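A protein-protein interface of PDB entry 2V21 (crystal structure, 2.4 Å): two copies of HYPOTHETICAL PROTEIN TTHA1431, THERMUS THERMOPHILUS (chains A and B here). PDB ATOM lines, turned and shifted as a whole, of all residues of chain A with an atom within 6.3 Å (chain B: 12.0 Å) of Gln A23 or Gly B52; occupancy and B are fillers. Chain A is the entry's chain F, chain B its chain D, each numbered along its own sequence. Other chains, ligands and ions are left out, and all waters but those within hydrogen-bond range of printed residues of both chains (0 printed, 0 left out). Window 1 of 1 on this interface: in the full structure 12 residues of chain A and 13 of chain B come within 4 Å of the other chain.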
ATOM      1  N   LEU A  18     -10.808 -35.963 -27.912  1.00  0.00           N
ATOM      2  CA  LEU A  18     -11.351 -35.551 -26.617  1.00  0.00           C
ATOM      3  C   LEU A  18     -10.507 -34.464 -25.966  1.00  0.00           C
ATOM      4  O   LEU A  18     -11.057 -33.489 -25.449  1.00  0.00           O
ATOM      5  CB  LEU A  18     -11.464 -36.757 -25.682  1.00  0.00           C
ATOM      6  CG  LEU A  18     -12.414 -37.857 -26.152  1.00  0.00           C
ATOM      7  CD1 LEU A  18     -12.331 -39.059 -25.224  1.00  0.00           C
ATOM      8  CD2 LEU A  18     -13.839 -37.352 -26.229  1.00  0.00           C
ATOM      9  N   GLU A  19      -9.183 -34.634 -25.992  1.00  0.00           N
ATOM     10  CA  GLU A  19      -8.263 -33.629 -25.443  1.00  0.00           C
ATOM     11  C   GLU A  19      -8.415 -32.282 -26.139  1.00  0.00           C
ATOM     12  O   GLU A  19      -8.441 -31.250 -25.480  1.00  0.00           O
ATOM     13  CB  GLU A  19      -6.800 -34.083 -25.547  1.00  0.00           C
ATOM     14  CG  GLU A  19      -6.402 -35.163 -24.540  1.00  0.00           C
ATOM     15  CD  GLU A  19      -6.608 -36.580 -25.053  1.00  0.00           C
ATOM     16  OE1 GLU A  19      -7.177 -36.763 -26.152  1.00  0.00           O
ATOM     17  OE2 GLU A  19      -6.201 -37.527 -24.345  1.00  0.00           O
ATOM     18  N   ALA A  20      -8.514 -32.310 -27.468  1.00  0.00           N
ATOM     19  CA  ALA A  20      -8.672 -31.087 -28.269  1.00  0.00           C
ATOM     20  C   ALA A  20      -9.997 -30.386 -27.949  1.00  0.00           C
ATOM     21  O   ALA A  20     -10.064 -29.161 -27.872  1.00  0.00           O
ATOM     22  CB  ALA A  20      -8.579 -31.406 -29.753  1.00  0.00           C
ATOM     23  N   ALA A  21     -11.045 -31.178 -27.748  1.00  0.00           N
ATOM     24  CA  ALA A  21     -12.338 -30.650 -27.334  1.00  0.00           C
ATOM     25  C   ALA A  21     -12.240 -29.928 -25.974  1.00  0.00           C
ATOM     26  O   ALA A  21     -12.781 -28.832 -25.796  1.00  0.00           O
ATOM     27  CB  ALA A  21     -13.352 -31.770 -27.275  1.00  0.00           C
ATOM     28  N   ILE A  22     -11.536 -30.539 -25.026  1.00  0.00           N
ATOM     29  CA  ILE A  22     -11.312 -29.919 -23.723  1.00  0.00           C
ATOM     30  C   ILE A  22     -10.521 -28.632 -23.897  1.00  0.00           C
ATOM     31  O   ILE A  22     -10.887 -27.587 -23.368  1.00  0.00           O
ATOM     32  CB  ILE A  22     -10.582 -30.891 -22.750  1.00  0.00           C
ATOM     33  CG1 ILE A  22     -11.524 -32.051 -22.371  1.00  0.00           C
ATOM     34  CG2 ILE A  22     -10.100 -30.161 -21.501  1.00  0.00           C
ATOM     35  CD1 ILE A  22     -10.845 -33.211 -21.684  1.00  0.00           C
ATOM     36  N   GLN A  23      -9.444 -28.708 -24.665  1.00  0.00           N
ATOM     37  CA  GLN A  23      -8.581 -27.560 -24.871  1.00  0.00           C
ATOM     38  C   GLN A  23      -9.316 -26.394 -25.539  1.00  0.00           C
ATOM     39  O   GLN A  23      -9.055 -25.237 -25.206  1.00  0.00           O
ATOM     40  CB  GLN A  23      -7.341 -27.964 -25.681  1.00  0.00           C
ATOM     41  CG  GLN A  23      -6.413 -28.931 -24.937  1.00  0.00           C
ATOM     42  CD  GLN A  23      -5.386 -28.229 -24.067  1.00  0.00           C
ATOM     43  OE1 GLN A  23      -4.242 -28.666 -23.969  1.00  0.00           O
ATOM     44  NE2 GLN A  23      -5.785 -27.130 -23.447  1.00  0.00           N
ATOM     45  N   ALA A  24     -10.229 -26.691 -26.465  1.00  0.00           N
ATOM     46  CA  ALA A  24     -11.040 -25.647 -27.107  1.00  0.00           C
ATOM     47  C   ALA A  24     -11.889 -24.900 -26.069  1.00  0.00           C
ATOM     48  O   ALA A  24     -11.973 -23.681 -26.086  1.00  0.00           O
ATOM     49  CB  ALA A  24     -11.918 -26.238 -28.202  1.00  0.00           C
ATOM     50  N   ALA A  25     -12.500 -25.638 -25.149  1.00  0.00           N
ATOM     51  CA  ALA A  25     -13.281 -25.028 -24.065  1.00  0.00           C
ATOM     52  C   ALA A  25     -12.404 -24.129 -23.177  1.00  0.00           C
ATOM     53  O   ALA A  25     -12.781 -22.996 -22.860  1.00  0.00           O
ATOM     54  CB  ALA A  25     -13.966 -26.102 -23.231  1.00  0.00           C
ATOM     55  N   LEU A  26     -11.234 -24.639 -22.794  1.00  0.00           N
ATOM     56  CA  LEU A  26     -10.320 -23.903 -21.922  1.00  0.00           C
ATOM     57  C   LEU A  26      -9.728 -22.672 -22.603  1.00  0.00           C
ATOM     58  O   LEU A  26      -9.560 -21.631 -21.955  1.00  0.00           O
ATOM     59  CB  LEU A  26      -9.195 -24.810 -21.404  1.00  0.00           C
ATOM     60  CG  LEU A  26      -9.620 -25.984 -20.506  1.00  0.00           C
ATOM     61  CD1 LEU A  26      -8.406 -26.679 -19.899  1.00  0.00           C
ATOM     62  CD2 LEU A  26     -10.580 -25.520 -19.415  1.00  0.00           C
ATOM     63  N   ALA A  27      -9.426 -22.787 -23.898  1.00  0.00           N
ATOM     64  CA  ALA A  27      -8.918 -21.654 -24.674  1.00  0.00           C
ATOM     65  C   ALA A  27      -9.935 -20.514 -24.702  1.00  0.00           C
ATOM     66  O   ALA A  27      -9.581 -19.359 -24.474  1.00  0.00           O
ATOM     67  CB  ALA A  27      -8.553 -22.088 -26.106  1.00  0.00           C
ATOM     68  N   ARG A  28     -11.197 -20.835 -24.976  1.00  0.00           N
ATOM     69  CA  ARG A  28     -12.248 -19.818 -24.985  1.00  0.00           C
ATOM     70  C   ARG A  28     -12.491 -19.270 -23.583  1.00  0.00           C
ATOM     71  O   ARG A  28     -12.717 -18.078 -23.415  1.00  0.00           O
ATOM     72  CB  ARG A  28     -13.553 -20.375 -25.576  1.00  0.00           C
ATOM     73  CG  ARG A  28     -14.754 -19.408 -25.523  1.00  0.00           C
ATOM     74  CD  ARG A  28     -14.439 -18.048 -26.131  1.00  0.00           C
ATOM     75  NE  ARG A  28     -15.584 -17.142 -26.128  1.00  0.00           N
ATOM     76  CZ  ARG A  28     -16.014 -16.443 -25.076  1.00  0.00           C
ATOM     77  NH1 ARG A  28     -15.421 -16.536 -23.888  1.00  0.00           N
ATOM     78  NH2 ARG A  28     -17.065 -15.637 -25.211  1.00  0.00           N
ATOM     79  N   ARG A  30     -10.401 -18.828 -21.100  1.00  0.00           N
ATOM     80  CA  ARG A  30      -9.346 -17.941 -20.591  1.00  0.00           C
ATOM     81  C   ARG A  30      -9.318 -16.558 -21.248  1.00  0.00           C
ATOM     82  O   ARG A  30      -8.599 -15.672 -20.786  1.00  0.00           O
ATOM     83  CB  ARG A  30      -7.953 -18.598 -20.670  1.00  0.00           C
ATOM     84  CG  ARG A  30      -7.344 -18.741 -22.068  1.00  0.00           C
ATOM     85  CD  ARG A  30      -5.830 -18.963 -21.978  1.00  0.00           C
ATOM     86  NE  ARG A  30      -5.251 -19.423 -23.243  1.00  0.00           N
ATOM     87  CZ  ARG A  30      -5.245 -20.688 -23.676  1.00  0.00           C
ATOM     88  NH1 ARG A  30      -5.796 -21.671 -22.957  1.00  0.00           N
ATOM     89  NH2 ARG A  30      -4.684 -20.973 -24.850  1.00  0.00           N
ATOM     90  N   LEU A  60     -18.166 -29.896 -19.733  1.00  0.00           N
ATOM     91  CA  LEU A  60     -17.062 -29.635 -18.837  1.00  0.00           C
ATOM     92  C   LEU A  60     -17.459 -28.552 -17.851  1.00  0.00           C
ATOM     93  O   LEU A  60     -18.039 -27.534 -18.248  1.00  0.00           O
ATOM     94  CB  LEU A  60     -15.884 -29.110 -19.689  1.00  0.00           C
ATOM     95  CG  LEU A  60     -14.499 -29.228 -19.091  1.00  0.00           C
ATOM     96  CD1 LEU A  60     -14.293 -30.684 -18.700  1.00  0.00           C
ATOM     97  CD2 LEU A  60     -13.459 -28.781 -20.054  1.00  0.00           C
ATOM     98  N   SER B  14      -1.293 -37.046 -16.116  1.00  0.00           N
ATOM     99  CA  SER B  14      -0.389 -36.857 -17.235  1.00  0.00           C
ATOM    100  C   SER B  14      -0.633 -35.502 -17.884  1.00  0.00           C
ATOM    101  O   SER B  14      -1.764 -35.027 -17.930  1.00  0.00           O
ATOM    102  CB  SER B  14      -0.577 -37.964 -18.279  1.00  0.00           C
ATOM    103  OG  SER B  14       0.171 -37.697 -19.464  1.00  0.00           O
ATOM    104  N   GLU B  15       0.436 -34.904 -18.399  1.00  0.00           N
ATOM    105  CA  GLU B  15       0.358 -33.659 -19.145  1.00  0.00           C
ATOM    106  C   GLU B  15       0.014 -33.917 -20.622  1.00  0.00           C
ATOM    107  O   GLU B  15      -0.269 -32.978 -21.368  1.00  0.00           O
ATOM    108  CB  GLU B  15       1.693 -32.910 -19.041  1.00  0.00           C
ATOM    109  CG  GLU B  15       2.145 -32.644 -17.603  1.00  0.00           C
ATOM    110  CD  GLU B  15       3.348 -31.716 -17.516  1.00  0.00           C
ATOM    111  OE1 GLU B  15       4.321 -31.912 -18.277  1.00  0.00           O
ATOM    112  OE2 GLU B  15       3.325 -30.792 -16.676  1.00  0.00           O
ATOM    113  N   GLU B  16       0.033 -35.186 -21.031  1.00  0.00           N
ATOM    114  CA  GLU B  16      -0.092 -35.561 -22.439  1.00  0.00           C
ATOM    115  C   GLU B  16      -1.536 -35.798 -22.880  1.00  0.00           C
ATOM    116  O   GLU B  16      -1.976 -35.275 -23.914  1.00  0.00           O
ATOM    117  CB  GLU B  16       0.772 -36.801 -22.710  1.00  0.00           C
ATOM    118  CG  GLU B  16       2.260 -36.555 -22.385  1.00  0.00           C
ATOM    119  CD  GLU B  16       3.193 -37.630 -22.915  1.00  0.00           C
ATOM    120  OE1 GLU B  16       4.208 -37.273 -23.548  1.00  0.00           O
ATOM    121  OE2 GLU B  16       2.922 -38.827 -22.690  1.00  0.00           O
ATOM    122  N   GLY B  17      -2.268 -36.582 -22.100  1.00  0.00           N
ATOM    123  CA  GLY B  17      -3.638 -36.911 -22.449  1.00  0.00           C
ATOM    124  C   GLY B  17      -4.254 -37.954 -21.544  1.00  0.00           C
ATOM    125  O   GLY B  17      -3.662 -38.346 -20.544  1.00  0.00           O
ATOM    126  N   LEU B  18      -5.444 -38.412 -21.920  1.00  0.00           N
ATOM    127  CA  LEU B  18      -6.256 -39.297 -21.082  1.00  0.00           C
ATOM    128  C   LEU B  18      -5.700 -40.717 -21.030  1.00  0.00           C
ATOM    129  O   LEU B  18      -5.624 -41.313 -19.950  1.00  0.00           O
ATOM    130  CB  LEU B  18      -7.703 -39.321 -21.580  1.00  0.00           C
ATOM    131  CG  LEU B  18      -8.435 -37.971 -21.516  1.00  0.00           C
ATOM    132  CD1 LEU B  18      -9.810 -38.039 -22.182  1.00  0.00           C
ATOM    133  CD2 LEU B  18      -8.555 -37.487 -20.067  1.00  0.00           C
ATOM    134  N   ILE B  44     -13.052 -37.975 -14.962  1.00  0.00           N
ATOM    135  CA  ILE B  44     -12.006 -37.276 -15.699  1.00  0.00           C
ATOM    136  C   ILE B  44     -12.041 -35.817 -15.241  1.00  0.00           C
ATOM    137  O   ILE B  44     -13.079 -35.147 -15.308  1.00  0.00           O
ATOM    138  CB  ILE B  44     -12.215 -37.365 -17.220  1.00  0.00           C
ATOM    139  CG1 ILE B  44     -12.113 -38.823 -17.695  1.00  0.00           C
ATOM    140  CG2 ILE B  44     -11.197 -36.494 -17.949  1.00  0.00           C
ATOM    141  CD1 ILE B  44     -12.669 -39.052 -19.077  1.00  0.00           C
ATOM    142  N   ARG B  45     -10.911 -35.353 -14.724  1.00  0.00           N
ATOM    143  CA  ARG B  45     -10.748 -33.956 -14.354  1.00  0.00           C
ATOM    144  C   ARG B  45      -9.323 -33.503 -14.659  1.00  0.00           C
ATOM    145  O   ARG B  45      -8.540 -34.235 -15.273  1.00  0.00           O
ATOM    146  CB  ARG B  45     -11.141 -33.738 -12.882  1.00  0.00           C
ATOM    147  CG  ARG B  45     -10.641 -34.767 -11.880  1.00  0.00           C
ATOM    148  CD  ARG B  45     -11.539 -34.790 -10.618  1.00  0.00           C
ATOM    149  NE  ARG B  45     -11.623 -33.473  -9.988  1.00  0.00           N
ATOM    150  CZ  ARG B  45     -12.626 -33.039  -9.220  1.00  0.00           C
ATOM    151  NH1 ARG B  45     -13.672 -33.812  -8.963  1.00  0.00           N
ATOM    152  NH2 ARG B  45     -12.589 -31.816  -8.701  1.00  0.00           N
ATOM    153  N   GLY B  46      -8.993 -32.281 -14.273  1.00  0.00           N
ATOM    154  CA  GLY B  46      -7.642 -31.793 -14.468  1.00  0.00           C
ATOM    155  C   GLY B  46      -7.423 -30.387 -13.969  1.00  0.00           C
ATOM    156  O   GLY B  46      -8.357 -29.704 -13.525  1.00  0.00           O
ATOM    157  N   THR B  47      -6.164 -29.966 -14.039  1.00  0.00           N
ATOM    158  CA  THR B  47      -5.770 -28.616 -13.656  1.00  0.00           C
ATOM    159  C   THR B  47      -5.555 -27.782 -14.901  1.00  0.00           C
ATOM    160  O   THR B  47      -5.285 -28.318 -15.983  1.00  0.00           O
ATOM    161  CB  THR B  47      -4.488 -28.624 -12.821  1.00  0.00           C
ATOM    162  OG1 THR B  47      -3.452 -29.305 -13.538  1.00  0.00           O
ATOM    163  CG2 THR B  47      -4.738 -29.322 -11.483  1.00  0.00           C
ATOM    164  N   ILE B  48      -5.700 -26.471 -14.739  1.00  0.00           N
ATOM    165  CA  ILE B  48      -5.597 -25.528 -15.845  1.00  0.00           C
ATOM    166  C   ILE B  48      -4.397 -24.627 -15.611  1.00  0.00           C
ATOM    167  O   ILE B  48      -4.189 -24.136 -14.499  1.00  0.00           O
ATOM    168  CB  ILE B  48      -6.869 -24.661 -15.962  1.00  0.00           C
ATOM    169  CG1 ILE B  48      -8.110 -25.545 -16.142  1.00  0.00           C
ATOM    170  CG2 ILE B  48      -6.744 -23.674 -17.122  1.00  0.00           C
ATOM    171  CD1 ILE B  48      -9.424 -24.786 -16.064  1.00  0.00           C
ATOM    172  N   GLY B  49      -3.610 -24.430 -16.666  1.00  0.00           N
ATOM    173  CA  GLY B  49      -2.464 -23.517 -16.645  1.00  0.00           C
ATOM    174  C   GLY B  49      -2.606 -22.433 -17.696  1.00  0.00           C
ATOM    175  O   GLY B  49      -3.678 -22.241 -18.266  1.00  0.00           O
ATOM    176  N   GLU B  50      -1.511 -21.725 -17.951  1.00  0.00           N
ATOM    177  CA  GLU B  50      -1.498 -20.611 -18.906  1.00  0.00           C
ATOM    178  C   GLU B  50      -1.747 -21.050 -20.353  1.00  0.00           C
ATOM    179  O   GLU B  50      -2.252 -20.271 -21.158  1.00  0.00           O
ATOM    180  N   ALA B  51      -1.403 -22.301 -20.666  1.00  0.00           N
ATOM    181  CA  ALA B  51      -1.575 -22.858 -22.010  1.00  0.00           C
ATOM    182  C   ALA B  51      -2.708 -23.894 -22.076  1.00  0.00           C
ATOM    183  O   ALA B  51      -2.687 -24.799 -22.912  1.00  0.00           O
ATOM    184  CB  ALA B  51      -0.257 -23.476 -22.488  1.00  0.00           C
ATOM    185  N   GLY B  52      -3.702 -23.751 -21.205  1.00  0.00           N
ATOM    186  CA  GLY B  52      -4.836 -24.672 -21.173  1.00  0.00           C
ATOM    187  C   GLY B  52      -4.639 -25.791 -20.162  1.00  0.00           C
ATOM    188  O   GLY B  52      -4.225 -25.543 -19.029  1.00  0.00           O
ATOM    189  N   VAL B  53      -4.934 -27.026 -20.564  1.00  0.00           N
ATOM    190  CA  VAL B  53      -4.732 -28.175 -19.687  1.00  0.00           C
ATOM    191  C   VAL B  53      -3.274 -28.242 -19.230  1.00  0.00           C
ATOM    192  O   VAL B  53      -2.336 -28.277 -20.039  1.00  0.00           O
ATOM    193  CB  VAL B  53      -5.114 -29.524 -20.340  1.00  0.00           C
ATOM    194  CG1 VAL B  53      -4.776 -30.663 -19.397  1.00  0.00           C
ATOM    195  CG2 VAL B  53      -6.602 -29.564 -20.706  1.00  0.00           C
ATOM    196  N   LYS B  54      -3.102 -28.214 -17.917  1.00  0.00           N
ATOM    197  CA  LYS B  54      -1.811 -28.399 -17.290  1.00  0.00           C
ATOM    198  C   LYS B  54      -1.640 -29.901 -17.086  1.00  0.00           C
ATOM    199  O   LYS B  54      -0.691 -30.505 -17.589  1.00  0.00           O
ATOM    200  CB  LYS B  54      -1.801 -27.645 -15.957  1.00  0.00           C
ATOM    201  CG  LYS B  54      -0.491 -27.632 -15.196  1.00  0.00           C
ATOM    202  CD  LYS B  54      -0.722 -27.081 -13.786  1.00  0.00           C
ATOM    203  CE  LYS B  54       0.565 -26.601 -13.144  1.00  0.00           C
ATOM    204  NZ  LYS B  54       0.329 -25.982 -11.806  1.00  0.00           N
ATOM    205  N   GLU B  55      -2.598 -30.501 -16.393  1.00  0.00           N
ATOM    206  CA  GLU B  55      -2.537 -31.908 -16.019  1.00  0.00           C
ATOM    207  C   GLU B  55      -3.899 -32.560 -16.204  1.00  0.00           C
ATOM    208  O   GLU B  55      -4.897 -32.046 -15.703  1.00  0.00           O
ATOM    209  CB  GLU B  55      -2.135 -32.001 -14.553  1.00  0.00           C
ATOM    210  CG  GLU B  55      -1.531 -33.303 -14.145  1.00  0.00           C
ATOM    211  CD  GLU B  55      -0.993 -33.240 -12.732  1.00  0.00           C
ATOM    212  OE1 GLU B  55      -1.800 -33.405 -11.783  1.00  0.00           O
ATOM    213  OE2 GLU B  55       0.232 -33.022 -12.577  1.00  0.00           O
ATOM    214  N   TYR B  56      -3.939 -33.671 -16.938  1.00  0.00           N
ATOM    215  CA  TYR B  56      -5.131 -34.518 -17.001  1.00  0.00           C
ATOM    216  C   TYR B  56      -5.129 -35.469 -15.821  1.00  0.00           C
ATOM    217  O   TYR B  56      -4.101 -36.042 -15.507  1.00  0.00           O
ATOM    218  CB  TYR B  56      -5.151 -35.341 -18.285  1.00  0.00           C
ATOM    219  CG  TYR B  56      -5.352 -34.529 -19.542  1.00  0.00           C
ATOM    220  CD1 TYR B  56      -4.276 -34.131 -20.311  1.00  0.00           C
ATOM    221  CD2 TYR B  56      -6.631 -34.176 -19.963  1.00  0.00           C
ATOM    222  CE1 TYR B  56      -4.463 -33.388 -21.472  1.00  0.00           C
ATOM    223  CE2 TYR B  56      -6.828 -33.443 -21.118  1.00  0.00           C
ATOM    224  CZ  TYR B  56      -5.749 -33.055 -21.865  1.00  0.00           C
ATOM    225  OH  TYR B  56      -5.978 -32.321 -22.994  1.00  0.00           O
ATOM    226  N   GLN B  57      -6.274 -35.630 -15.170  1.00  0.00           N
ATOM    227  CA  GLN B  57      -6.396 -36.507 -14.001  1.00  0.00           C
ATOM    228  C   GLN B  57      -7.555 -37.487 -14.183  1.00  0.00           C
ATOM    229  O   GLN B  57      -8.721 -37.087 -14.255  1.00  0.00           O
ATOM    230  CB  GLN B  57      -6.603 -35.683 -12.728  1.00  0.00           C
ATOM    231  CG  GLN B  57      -5.451 -34.698 -12.439  1.00  0.00           C
ATOM    232  CD  GLN B  57      -5.781 -33.643 -11.381  1.00  0.00           C
ATOM    233  OE1 GLN B  57      -4.879 -33.078 -10.759  1.00  0.00           O
ATOM    234  NE2 GLN B  57      -7.064 -33.370 -11.179  1.00  0.00           N
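N of Leu B18 lies within hydrogen-bond range of OE2 of Glu A19, 2.7 Å away. N of Val B53 sits close to NE2 of Gln A23, 3.0 Å away. NH1 of Arg A30 sits close to N of Gly B52 (3.4 Å).
O of Ser B14 sits at hydrogen-bond distance from N of Tyr B56, 2.7 Å away.
Among the printed residues, merely in contact across the chains: Glu A19 with Gly B17 (3.2 Å), Glu A19 with Tyr B56 (3.2 Å), Ile A22 with Val B53 (3.6 Å), Gln A23 with Ala B51 (3.9 Å), Gln A23 with Gly B52 (3.5 Å), Gln A23 with Tyr B56 (3.9 Å), Leu A26 with Ile B48 (3.6 Å), Leu A26 with Gly B52 (3.9 Å), Leu A26 with Val B53 (3.5 Å), Arg A30 with Glu B50 (3.7 Å) and Arg A30 with Ala B51 (3.9 Å).
Of the printed residues of chain B, Gln A23 touches Ala B51, Gly B52, Val B53 and Tyr B56. Of chain A, only Gln A23 (3.5 Å), Leu A26 (3.9 Å) and Arg A30 (3.4 Å) come within 4 Å of Gly B52. No residue of chain B comes within 4 Å of Ala A21. Of chain B, only Val B53 comes within 4 Å of Ile A22. Ala A24 touches none of the printed residues of chain B. No residue of chain B comes within 4 Å of Ala A25. Printed residues of chain B within 4 Å of Leu A26: Ile B48 (3.6 Å), Gly B52 (3.9 Å) and Val B53 (3.5 Å). Of the printed residues of chain A, Gly B17 touches Glu A19 (3.2 Å). Of the printed residues of chain A, Val B53 touches Ile A22 (3.6 Å), Gln A23 (3.0 Å) and Leu A26 (3.5 Å). Of the printed residues of chain A, Leu B18 touches Glu A19 (2.7 Å).
Hydrophobic or aromatic side chains of chain B within 4 Å of the printed part of chain A: Leu B18, Ile B48, Val B53 and Tyr B56. Of the 13 printed residues of chain A, 5 touch a printed residue of chain B. Along chain A the printed residues that touch a printed residue of chain B span positions 19 to 30.
1 position is printed for both chains. Of the 14 pairs that touch across the chains among the printed residues, none has its exchanged pair printed and touching as well.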
